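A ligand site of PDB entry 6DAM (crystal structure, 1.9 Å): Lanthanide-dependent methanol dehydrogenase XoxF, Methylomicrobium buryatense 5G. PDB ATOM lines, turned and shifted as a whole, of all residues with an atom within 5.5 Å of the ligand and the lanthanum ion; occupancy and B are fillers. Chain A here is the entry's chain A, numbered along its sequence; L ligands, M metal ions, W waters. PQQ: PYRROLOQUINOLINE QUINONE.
Within 4 Å of the lanthanum ion: Glu 197, Asn 285, Asp 327 and Asp 329. Along chain A the residues within 4 Å of the lanthanum ion span positions 197 to 329.
The side-chain sulfur (SG) of Cys 130 is disulfide-bonded to the side-chain sulfur (SG) of Cys 129 (2.1 Å). The side-chain carboxylate of Glu 81 lies close to the side-chain amide oxygen of Gln 421, at 3.5 Å. The side-chain carboxylate of Asp 327 lies within salt-bridge range of the guanidinium group of Arg 354, 3.3 Å away. The backbone carbonyl oxygen (O) of Thr 179 sits at hydrogen-bond distance from the backbone NH (N) of Arg 135. The guanidinium group (NE) of Arg 354 sits close to the backbone carbonyl oxygen (O) of Leu 416 (3.4 Å). The backbone NH (N) of Ser 194 sits at hydrogen-bond distance from the backbone carbonyl oxygen (O) of Thr 177. The side-chain hydroxyl of Thr 179 is in hydrogen-bond range of the side-chain hydroxyl of Ser 194 (3.3 Å). The side-chain carboxylate (OD1) of Asp 329 sits close to the guanidinium group (NH2) of Arg 354, at 3.4 Å.
O7A of the ligand is bound to the lanthanum ion. The lanthanum ion is bound by OD1 of Asp 329 (2.5 Å). OD1 of Asn 285 is bound to the lanthanum ion (2.6 Å). The lanthanum ion is bound by OE1 of Glu 197. An oxygen (O5) of the ligand is bound to the lanthanum ion. The side-chain carboxylate (OD2) of Asp 329 binds the lanthanum ion (2.7 Å). The lanthanum ion is bound by OE2 of Glu 197. OD1 of Asp 327 binds the lanthanum ion (2.8 Å). The lanthanum ion is bound by a nitrogen (N6) of the ligand, at 2.8 Å. The lanthanum ion has nine donor atoms within binding distance.
An oxygen (O2B) of the ligand lies within hydrogen-bond range of the backbone NH (N) of Trp 570 (2.5 Å). NH2 of Arg 135 is in salt-bridge range of O9B of the ligand. The indole nitrogen of Trp 267 lies close to a nitrogen (N6) of the ligand (3.4 Å). The side-chain hydroxyl (OG1) of Thr 265 lies within hydrogen-bond range of an oxygen (O7B) of the ligand (2.7 Å). The side-chain amide nitrogen of Asn 420 is in hydrogen-bond range of an oxygen (O4) of the ligand (3.3 Å). The side-chain hydroxyl of Ser 194 is in hydrogen-bond range of an oxygen (O9A) of the ligand (2.7 Å). An oxygen (O2A) of the ligand sits close to the side-chain carboxylate of Glu 81. The backbone NH (N) of Gly 196 is in hydrogen-bond range of an oxygen (O7B) of the ligand (2.6 Å). An oxygen (O4) of the ligand sits at hydrogen-bond distance from the guanidinium group of Arg 354, 3.1 Å away. The indole nitrogen (NE1) of Trp 506 is in hydrogen-bond range of an oxygen (O2B) of the ligand. N of Gly 195 lies within hydrogen-bond range of O7B of the ligand (2.8 Å). The side-chain hydroxyl of Thr 179 lies within hydrogen-bond range of an oxygen (O9A) of the ligand.
Water W1 lies within hydrogen-bond range of OG1 of Thr 177 (2.9 Å) and O9A of the ligand (3.0 Å). Water W4 lies within hydrogen-bond range of the side-chain carboxylate of Asp 327 (2.5 Å), an oxygen (O4) of the ligand (3.1 Å) and the guanidinium group of Arg 354 (3.3 Å). Water W3 lies within hydrogen-bond range of the backbone NH (N) of Glu 197 (2.9 Å), an oxygen (O7B) of the ligand (3.2 Å), the backbone NH (N) of Gly 196 (3.2 Å) and the side-chain sulfur (SG) of Cys 129 (3.7 Å). Water W2 bridges the side-chain hydroxyl of Thr 265 and the backbone carbonyl oxygen of Asn 285.
Cys 129 touches the ligand. Cys 130 touches the ligand (CB to N1, 3.5 Å). Val 133 touches the ligand (CG2 to O2A, 3.9 Å). CA of Gly 569 touches O2B of the ligand (3.2 Å). 20 residues have an atom within 4 Å of the ligand: Glu 81, Cys 129, Cys 130, Val 133, Arg 135, Thr 179, Ser 194, Gly 195, Gly 196, Glu 197, Thr 265, Trp 267, Asn 285, Asp 327, Asp 329, Arg 354, Asn 420, Trp 506, Gly 569 and Trp 570. The nearest printed residue that does not touch the ligand is Gln 421 (4.04 Å).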
ATOM      1  N   GLU A  81      12.608  -6.890  14.856  1.00  0.00           N
ATOM      2  CA  GLU A  81      12.450  -7.321  13.478  1.00  0.00           C
ATOM      3  C   GLU A  81      13.767  -7.115  12.710  1.00  0.00           C
ATOM      4  O   GLU A  81      14.765  -6.607  13.248  1.00  0.00           O
ATOM      5  CB  GLU A  81      11.264  -6.592  12.814  1.00  0.00           C
ATOM      6  CG  GLU A  81       9.916  -7.006  13.412  1.00  0.00           C
ATOM      7  CD  GLU A  81       8.674  -6.427  12.730  1.00  0.00           C
ATOM      8  OE1 GLU A  81       7.544  -6.717  13.201  1.00  0.00           O
ATOM      9  OE2 GLU A  81       8.816  -5.703  11.722  1.00  0.00           O
ATOM     10  N   CYS A 129       1.600   2.280  15.047  1.00  0.00           N
ATOM     11  CA  CYS A 129       0.481   1.382  15.081  1.00  0.00           C
ATOM     12  C   CYS A 129       0.677  -0.021  15.586  1.00  0.00           C
ATOM     13  O   CYS A 129      -0.232  -0.582  16.138  1.00  0.00           O
ATOM     14  CB  CYS A 129      -0.063   1.198  13.654  1.00  0.00           C
ATOM     15  SG  CYS A 129       0.895   0.049  12.625  1.00  0.00           S
ATOM     16  N   CYS A 130       1.875  -0.526  15.463  1.00  0.00           N
ATOM     17  CA  CYS A 130       2.085  -1.966  15.528  1.00  0.00           C
ATOM     18  C   CYS A 130       3.450  -2.294  16.113  1.00  0.00           C
ATOM     19  O   CYS A 130       4.250  -3.013  15.519  1.00  0.00           O
ATOM     20  CB  CYS A 130       1.912  -2.558  14.121  1.00  0.00           C
ATOM     21  SG  CYS A 130       0.437  -1.921  13.192  1.00  0.00           S
ATOM     22  N   VAL A 133       8.982  -1.402  16.316  1.00  0.00           N
ATOM     23  CA  VAL A 133       9.922  -2.169  15.531  1.00  0.00           C
ATOM     24  C   VAL A 133      10.692  -1.390  14.468  1.00  0.00           C
ATOM     25  O   VAL A 133      10.293  -0.374  14.065  1.00  0.00           O
ATOM     26  CB  VAL A 133       9.185  -3.318  14.863  1.00  0.00           C
ATOM     27  CG1 VAL A 133       8.568  -4.280  15.863  1.00  0.00           C
ATOM     28  CG2 VAL A 133       8.179  -2.799  13.882  1.00  0.00           C
ATOM     29  N   ARG A 135      12.928  -2.543  10.857  1.00  0.00           N
ATOM     30  CA  ARG A 135      13.272  -3.631   9.980  1.00  0.00           C
ATOM     31  C   ARG A 135      14.709  -3.761   9.540  1.00  0.00           C
ATOM     32  O   ARG A 135      15.051  -4.646   8.839  1.00  0.00           O
ATOM     33  CB  ARG A 135      12.253  -3.823   8.834  1.00  0.00           C
ATOM     34  CG  ARG A 135      10.888  -4.209   9.385  1.00  0.00           C
ATOM     35  CD  ARG A 135       9.783  -4.560   8.397  1.00  0.00           C
ATOM     36  NE  ARG A 135       8.647  -4.522   9.241  1.00  0.00           N
ATOM     37  CZ  ARG A 135       7.968  -3.442   9.525  1.00  0.00           C
ATOM     38  NH1 ARG A 135       8.211  -2.361   8.856  1.00  0.00           N
ATOM     39  NH2 ARG A 135       7.042  -3.469  10.437  1.00  0.00           N
ATOM     40  N   THR A 177       5.286   7.624  10.709  1.00  0.00           N
ATOM     41  CA  THR A 177       6.411   6.960  11.362  1.00  0.00           C
ATOM     42  C   THR A 177       7.176   6.183  10.308  1.00  0.00           C
ATOM     43  O   THR A 177       6.761   6.093   9.143  1.00  0.00           O
ATOM     44  CB  THR A 177       5.954   6.019  12.492  1.00  0.00           C
ATOM     45  OG1 THR A 177       5.039   5.038  11.969  1.00  0.00           O
ATOM     46  CG2 THR A 177       5.279   6.802  13.600  1.00  0.00           C
ATOM     47  N   THR A 179       9.131   2.303  10.089  1.00  0.00           N
ATOM     48  CA  THR A 179       9.515   1.041  10.678  1.00  0.00           C
ATOM     49  C   THR A 179      10.330   0.177   9.732  1.00  0.00           C
ATOM     50  O   THR A 179      10.861  -0.847  10.153  1.00  0.00           O
ATOM     51  CB  THR A 179       8.261   0.257  11.116  1.00  0.00           C
ATOM     52  OG1 THR A 179       7.385   0.107   9.996  1.00  0.00           O
ATOM     53  CG2 THR A 179       7.542   1.007  12.224  1.00  0.00           C
ATOM     54  N   ILE A 193       7.435   5.067   4.175  1.00  0.00           N
ATOM     55  CA  ILE A 193       6.722   5.706   5.278  1.00  0.00           C
ATOM     56  C   ILE A 193       5.659   4.731   5.792  1.00  0.00           C
ATOM     57  O   ILE A 193       5.217   3.827   5.071  1.00  0.00           O
ATOM     58  CB  ILE A 193       6.121   7.064   4.820  1.00  0.00           C
ATOM     59  CG1 ILE A 193       5.867   7.998   6.021  1.00  0.00           C
ATOM     60  CG2 ILE A 193       4.841   6.854   3.998  1.00  0.00           C
ATOM     61  CD1 ILE A 193       7.124   8.649   6.557  1.00  0.00           C
ATOM     62  N   SER A 194       5.261   4.902   7.057  1.00  0.00           N
ATOM     63  CA  SER A 194       4.138   4.194   7.665  1.00  0.00           C
ATOM     64  C   SER A 194       3.071   5.180   8.113  1.00  0.00           C
ATOM     65  O   SER A 194       3.349   6.356   8.370  1.00  0.00           O
ATOM     66  CB  SER A 194       4.564   3.367   8.898  1.00  0.00           C
ATOM     67  OG  SER A 194       5.450   2.337   8.524  1.00  0.00           O
ATOM     68  N   GLY A 195       1.839   4.684   8.237  1.00  0.00           N
ATOM     69  CA  GLY A 195       0.744   5.525   8.698  1.00  0.00           C
ATOM     70  C   GLY A 195      -0.582   5.276   8.013  1.00  0.00           C
ATOM     71  O   GLY A 195      -1.439   6.164   7.970  1.00  0.00           O
ATOM     72  N   GLY A 196      -0.769   4.067   7.467  1.00  0.00           N
ATOM     73  CA  GLY A 196      -2.044   3.710   6.843  1.00  0.00           C
ATOM     74  C   GLY A 196      -3.201   3.571   7.821  1.00  0.00           C
ATOM     75  O   GLY A 196      -4.357   3.476   7.376  1.00  0.00           O
ATOM     76  N   GLU A 197      -2.920   3.568   9.113  1.00  0.00           N
ATOM     77  CA  GLU A 197      -3.971   3.634  10.128  1.00  0.00           C
ATOM     78  C   GLU A 197      -4.094   5.045  10.709  1.00  0.00           C
ATOM     79  O   GLU A 197      -4.888   5.252  11.643  1.00  0.00           O
ATOM     80  CB  GLU A 197      -3.699   2.603  11.236  1.00  0.00           C
ATOM     81  CG  GLU A 197      -4.167   1.170  10.896  1.00  0.00           C
ATOM     82  CD  GLU A 197      -3.406   0.550   9.733  1.00  0.00           C
ATOM     83  OE1 GLU A 197      -3.969   0.456   8.603  1.00  0.00           O
ATOM     84  OE2 GLU A 197      -2.238   0.132   9.934  1.00  0.00           O
ATOM     85  N   THR A 265       0.712   3.240   2.145  1.00  0.00           N
ATOM     86  CA  THR A 265       2.034   3.454   2.706  1.00  0.00           C
ATOM     87  C   THR A 265       2.966   2.318   2.260  1.00  0.00           C
ATOM     88  O   THR A 265       2.565   1.378   1.573  1.00  0.00           O
ATOM     89  CB  THR A 265       1.969   3.590   4.234  1.00  0.00           C
ATOM     90  OG1 THR A 265       1.389   2.403   4.800  1.00  0.00           O
ATOM     91  CG2 THR A 265       1.122   4.790   4.646  1.00  0.00           C
ATOM     92  N   TRP A 267       5.783   0.366   3.986  1.00  0.00           N
ATOM     93  CA  TRP A 267       6.544  -0.082   5.136  1.00  0.00           C
ATOM     94  C   TRP A 267       7.084  -1.496   4.966  1.00  0.00           C
ATOM     95  O   TRP A 267       7.565  -2.094   5.946  1.00  0.00           O
ATOM     96  CB  TRP A 267       5.687   0.017   6.410  1.00  0.00           C
ATOM     97  CG  TRP A 267       4.377  -0.710   6.322  1.00  0.00           C
ATOM     98  CD1 TRP A 267       3.224  -0.274   5.726  1.00  0.00           C
ATOM     99  CD2 TRP A 267       4.068  -2.000   6.876  1.00  0.00           C
ATOM    100  NE1 TRP A 267       2.232  -1.223   5.837  1.00  0.00           N
ATOM    101  CE2 TRP A 267       2.726  -2.293   6.552  1.00  0.00           C
ATOM    102  CE3 TRP A 267       4.810  -2.946   7.595  1.00  0.00           C
ATOM    103  CZ2 TRP A 267       2.094  -3.483   6.919  1.00  0.00           C
ATOM    104  CZ3 TRP A 267       4.175  -4.141   7.975  1.00  0.00           C
ATOM    105  CH2 TRP A 267       2.826  -4.397   7.632  1.00  0.00           C
ATOM    106  N   ASN A 285      -2.722  -0.193   2.739  1.00  0.00           N
ATOM    107  CA  ASN A 285      -4.167  -0.056   2.706  1.00  0.00           C
ATOM    108  C   ASN A 285      -4.584   1.383   2.446  1.00  0.00           C
ATOM    109  O   ASN A 285      -3.860   2.325   2.809  1.00  0.00           O
ATOM    110  CB  ASN A 285      -4.769  -0.524   4.025  1.00  0.00           C
ATOM    111  CG  ASN A 285      -4.304   0.321   5.187  1.00  0.00           C
ATOM    112  OD1 ASN A 285      -3.137   0.234   5.600  1.00  0.00           O
ATOM    113  ND2 ASN A 285      -5.187   1.142   5.726  1.00  0.00           N
ATOM    114  N   TRP A 289     -10.460   1.965   7.598  1.00  0.00           N
ATOM    115  CA  TRP A 289     -10.853   0.564   7.513  1.00  0.00           C
ATOM    116  C   TRP A 289     -12.333   0.397   7.232  1.00  0.00           C
ATOM    117  O   TRP A 289     -12.820  -0.737   7.225  1.00  0.00           O
ATOM    118  CB  TRP A 289     -10.509  -0.170   8.804  1.00  0.00           C
ATOM    119  CG  TRP A 289      -9.054  -0.366   9.058  1.00  0.00           C
ATOM    120  CD1 TRP A 289      -8.025   0.366   8.525  1.00  0.00           C
ATOM    121  CD2 TRP A 289      -8.455  -1.335   9.922  1.00  0.00           C
ATOM    122  NE1 TRP A 289      -6.825  -0.095   9.004  1.00  0.00           N
ATOM    123  CE2 TRP A 289      -7.067  -1.139   9.867  1.00  0.00           C
ATOM    124  CE3 TRP A 289      -8.969  -2.341  10.740  1.00  0.00           C
ATOM    125  CZ2 TRP A 289      -6.165  -1.925  10.593  1.00  0.00           C
ATOM    126  CZ3 TRP A 289      -8.078  -3.123  11.472  1.00  0.00           C
ATOM    127  CH2 TRP A 289      -6.690  -2.918  11.383  1.00  0.00           C
ATOM    128  N   ASP A 327      -7.982  -4.234   5.360  1.00  0.00           N
ATOM    129  CA  ASP A 327      -6.594  -3.855   5.706  1.00  0.00           C
ATOM    130  C   ASP A 327      -5.571  -4.916   5.281  1.00  0.00           C
ATOM    131  O   ASP A 327      -4.615  -5.225   6.008  1.00  0.00           O
ATOM    132  CB  ASP A 327      -6.432  -3.550   7.205  1.00  0.00           C
ATOM    133  CG  ASP A 327      -5.092  -2.880   7.503  1.00  0.00           C
ATOM    134  OD1 ASP A 327      -4.764  -1.902   6.819  1.00  0.00           O
ATOM    135  OD2 ASP A 327      -4.349  -3.337   8.411  1.00  0.00           O
ATOM    136  N   ASP A 329      -2.799  -4.916   3.642  1.00  0.00           N
ATOM    137  CA  ASP A 329      -1.701  -4.113   3.106  1.00  0.00           C
ATOM    138  C   ASP A 329      -0.905  -4.861   2.047  1.00  0.00           C
ATOM    139  O   ASP A 329      -0.460  -5.988   2.275  1.00  0.00           O
ATOM    140  CB  ASP A 329      -0.733  -3.693   4.216  1.00  0.00           C
ATOM    141  CG  ASP A 329      -1.323  -2.689   5.190  1.00  0.00           C
ATOM    142  OD1 ASP A 329      -2.379  -2.969   5.792  1.00  0.00           O
ATOM    143  OD2 ASP A 329      -0.708  -1.615   5.388  1.00  0.00           O
ATOM    144  N   ARG A 354      -0.624 -10.061   1.870  1.00  0.00           N
ATOM    145  CA  ARG A 354      -1.503 -10.151   3.040  1.00  0.00           C
ATOM    146  C   ARG A 354      -2.841 -10.783   2.695  1.00  0.00           C
ATOM    147  O   ARG A 354      -3.406 -11.506   3.523  1.00  0.00           O
ATOM    148  CB  ARG A 354      -1.728  -8.758   3.630  1.00  0.00           C
ATOM    149  CG  ARG A 354      -0.504  -8.248   4.397  1.00  0.00           C
ATOM    150  CD  ARG A 354      -0.640  -8.570   5.865  1.00  0.00           C
ATOM    151  NE  ARG A 354      -1.629  -7.706   6.507  1.00  0.00           N
ATOM    152  CZ  ARG A 354      -1.322  -6.527   7.044  1.00  0.00           C
ATOM    153  NH1 ARG A 354      -0.070  -6.087   6.987  1.00  0.00           N
ATOM    154  NH2 ARG A 354      -2.269  -5.782   7.616  1.00  0.00           N
ATOM    155  N   ALA A 415      -7.074  -9.413   9.258  1.00  0.00           N
ATOM    156  CA  ALA A 415      -6.395  -8.260   8.660  1.00  0.00           C
ATOM    157  C   ALA A 415      -4.878  -8.450   8.642  1.00  0.00           C
ATOM    158  O   ALA A 415      -4.204  -8.031   7.693  1.00  0.00           O
ATOM    159  CB  ALA A 415      -6.762  -6.976   9.416  1.00  0.00           C
ATOM    160  N   LEU A 416      -4.320  -9.096   9.682  1.00  0.00           N
ATOM    161  CA  LEU A 416      -2.877  -9.259   9.681  1.00  0.00           C
ATOM    162  C   LEU A 416      -2.388 -10.214   8.603  1.00  0.00           C
ATOM    163  O   LEU A 416      -1.159 -10.410   8.502  1.00  0.00           O
ATOM    164  CB  LEU A 416      -2.378  -9.699  11.064  1.00  0.00           C
ATOM    165  CG  LEU A 416      -3.014 -10.858  11.832  1.00  0.00           C
ATOM    166  CD1 LEU A 416      -2.701 -12.204  11.195  1.00  0.00           C
ATOM    167  CD2 LEU A 416      -2.516 -10.816  13.269  1.00  0.00           C
ATOM    168  N   ASN A 420       2.433 -11.682   6.930  1.00  0.00           N
ATOM    169  CA  ASN A 420       2.668 -10.282   7.260  1.00  0.00           C
ATOM    170  C   ASN A 420       4.084  -9.894   6.830  1.00  0.00           C
ATOM    171  O   ASN A 420       4.575 -10.404   5.815  1.00  0.00           O
ATOM    172  CB  ASN A 420       2.423 -10.041   8.751  1.00  0.00           C
ATOM    173  CG  ASN A 420       2.068  -8.598   9.060  1.00  0.00           C
ATOM    174  OD1 ASN A 420       2.941  -7.717   9.058  1.00  0.00           O
ATOM    175  ND2 ASN A 420       0.800  -8.344   9.331  1.00  0.00           N
ATOM    176  N   GLN A 421       4.756  -9.026   7.596  1.00  0.00           N
ATOM    177  CA  GLN A 421       6.038  -8.469   7.149  1.00  0.00           C
ATOM    178  C   GLN A 421       7.096  -9.540   6.898  1.00  0.00           C
ATOM    179  O   GLN A 421       7.969  -9.348   6.042  1.00  0.00           O
ATOM    180  CB  GLN A 421       6.577  -7.471   8.194  1.00  0.00           C
ATOM    181  CG  GLN A 421       6.745  -8.041   9.606  1.00  0.00           C
ATOM    182  CD  GLN A 421       8.131  -8.622   9.869  1.00  0.00           C
ATOM    183  OE1 GLN A 421       9.142  -8.161   9.283  1.00  0.00           O
ATOM    184  NE2 GLN A 421       8.207  -9.633  10.731  1.00  0.00           N
ATOM    185  N   TRP A 506       6.195 -15.490  12.378  1.00  0.00           N
ATOM    186  CA  TRP A 506       6.539 -14.103  12.182  1.00  0.00           C
ATOM    187  C   TRP A 506       8.022 -13.706  11.840  1.00  0.00           C
ATOM    188  O   TRP A 506       8.424 -12.590  11.960  1.00  0.00           O
ATOM    189  CB  TRP A 506       6.007 -13.271  13.372  1.00  0.00           C
ATOM    190  CG  TRP A 506       5.409 -11.991  13.070  1.00  0.00           C
ATOM    191  CD1 TRP A 506       6.004 -10.787  13.145  1.00  0.00           C
ATOM    192  CD2 TRP A 506       4.049 -11.719  12.720  1.00  0.00           C
ATOM    193  NE1 TRP A 506       5.123  -9.782  12.855  1.00  0.00           N
ATOM    194  CE2 TRP A 506       3.921 -10.338  12.564  1.00  0.00           C
ATOM    195  CE3 TRP A 506       2.916 -12.523  12.524  1.00  0.00           C
ATOM    196  CZ2 TRP A 506       2.720  -9.762  12.201  1.00  0.00           C
ATOM    197  CZ3 TRP A 506       1.760 -11.936  12.160  1.00  0.00           C
ATOM    198  CH2 TRP A 506       1.669 -10.579  11.995  1.00  0.00           C
ATOM    199  N   GLY A 568       7.201  -9.183  19.566  1.00  0.00           N
ATOM    200  CA  GLY A 568       6.579  -7.892  19.380  1.00  0.00           C
ATOM    201  C   GLY A 568       5.868  -7.814  18.038  1.00  0.00           C
ATOM    202  O   GLY A 568       5.444  -8.836  17.476  1.00  0.00           O
ATOM    203  N   GLY A 569       5.758  -6.595  17.516  1.00  0.00           N
ATOM    204  CA  GLY A 569       5.019  -6.428  16.259  1.00  0.00           C
ATOM    205  C   GLY A 569       3.558  -6.814  16.407  1.00  0.00           C
ATOM    206  O   GLY A 569       2.980  -6.729  17.495  1.00  0.00           O
ATOM    207  N   TRP A 570       2.980  -7.305  15.301  1.00  0.00           N
ATOM    208  CA  TRP A 570       1.556  -7.636  15.043  1.00  0.00           C
ATOM    209  C   TRP A 570       0.703  -6.398  14.799  1.00  0.00           C
ATOM    210  O   TRP A 570      -0.498  -6.517  14.561  1.00  0.00           O
ATOM    211  CB  TRP A 570       0.902  -8.451  16.156  1.00  0.00           C
ATOM    212  CG  TRP A 570       1.762  -9.453  16.754  1.00  0.00           C
ATOM    213  CD1 TRP A 570       2.403 -10.483  16.115  1.00  0.00           C
ATOM    214  CD2 TRP A 570       2.089  -9.566  18.144  1.00  0.00           C
ATOM    215  NE1 TRP A 570       3.124 -11.219  17.030  1.00  0.00           N
ATOM    216  CE2 TRP A 570       2.944 -10.669  18.287  1.00  0.00           C
ATOM    217  CE3 TRP A 570       1.754  -8.817  19.283  1.00  0.00           C
ATOM    218  CZ2 TRP A 570       3.462 -11.057  19.523  1.00  0.00           C
ATOM    219  CZ3 TRP A 570       2.263  -9.196  20.513  1.00  0.00           C
ATOM    220  CH2 TRP A 570       3.108 -10.307  20.627  1.00  0.00           C
HETATM  221  N1  PQQ L   1       3.515  -3.868  11.341  1.00  0.00           N
HETATM  222  C2  PQQ L   1       3.338  -5.140  11.823  1.00  0.00           C
HETATM  223  C2X PQQ L   1       4.446  -5.858  12.552  1.00  0.00           C
HETATM  224  O2A PQQ L   1       5.612  -5.369  12.418  1.00  0.00           O
HETATM  225  O2B PQQ L   1       4.236  -6.947  13.148  1.00  0.00           O
HETATM  226  C3  PQQ L   1       2.088  -5.614  11.446  1.00  0.00           C
HETATM  227  C3A PQQ L   1       1.485  -4.618  10.755  1.00  0.00           C
HETATM  228  C1A PQQ L   1       2.374  -3.514  10.691  1.00  0.00           C
HETATM  229  C4  PQQ L   1       0.132  -4.543  10.102  1.00  0.00           C
HETATM  230  O4  PQQ L   1      -0.599  -5.492  10.186  1.00  0.00           O
HETATM  231  C5  PQQ L   1      -0.257  -3.335   9.413  1.00  0.00           C
HETATM  232  O5  PQQ L   1      -1.319  -3.228   8.876  1.00  0.00           O
HETATM  233  C6A PQQ L   1       0.682  -2.170   9.345  1.00  0.00           C
HETATM  234  N6  PQQ L   1       0.313  -1.043   8.690  1.00  0.00           N
HETATM  235  C7  PQQ L   1       1.166   0.024   8.610  1.00  0.00           C
HETATM  236  C7X PQQ L   1       0.429   1.078   7.766  1.00  0.00           C
HETATM  237  O7A PQQ L   1      -0.701   0.836   7.236  1.00  0.00           O
HETATM  238  O7B PQQ L   1       1.043   2.146   7.509  1.00  0.00           O
HETATM  239  C8  PQQ L   1       2.443  -0.048   9.202  1.00  0.00           C
HETATM  240  C9  PQQ L   1       2.827  -1.184   9.873  1.00  0.00           C
HETATM  241  C9X PQQ L   1       4.231  -0.828  10.369  1.00  0.00           C
HETATM  242  O9A PQQ L   1       4.756   0.280  10.093  1.00  0.00           O
HETATM  243  O9B PQQ L   1       4.838  -1.635  11.129  1.00  0.00           O
HETATM  244  C9A PQQ L   1       1.962  -2.247   9.958  1.00  0.00           C
HETATM  245 LA    LA M   1      -2.221  -1.162   7.569  1.00  0.00          LA
HETATM  246  O   HOH W   1       4.408   2.223  12.318  1.00  0.00           O
HETATM  247  O   HOH W   2      -1.303   2.016   4.011  1.00  0.00           O
HETATM  248  O   HOH W   3      -0.517   2.544  10.273  1.00  0.00           O
HETATM  249  O   HOH W   4      -3.528  -4.662  10.412  1.00  0.00           O
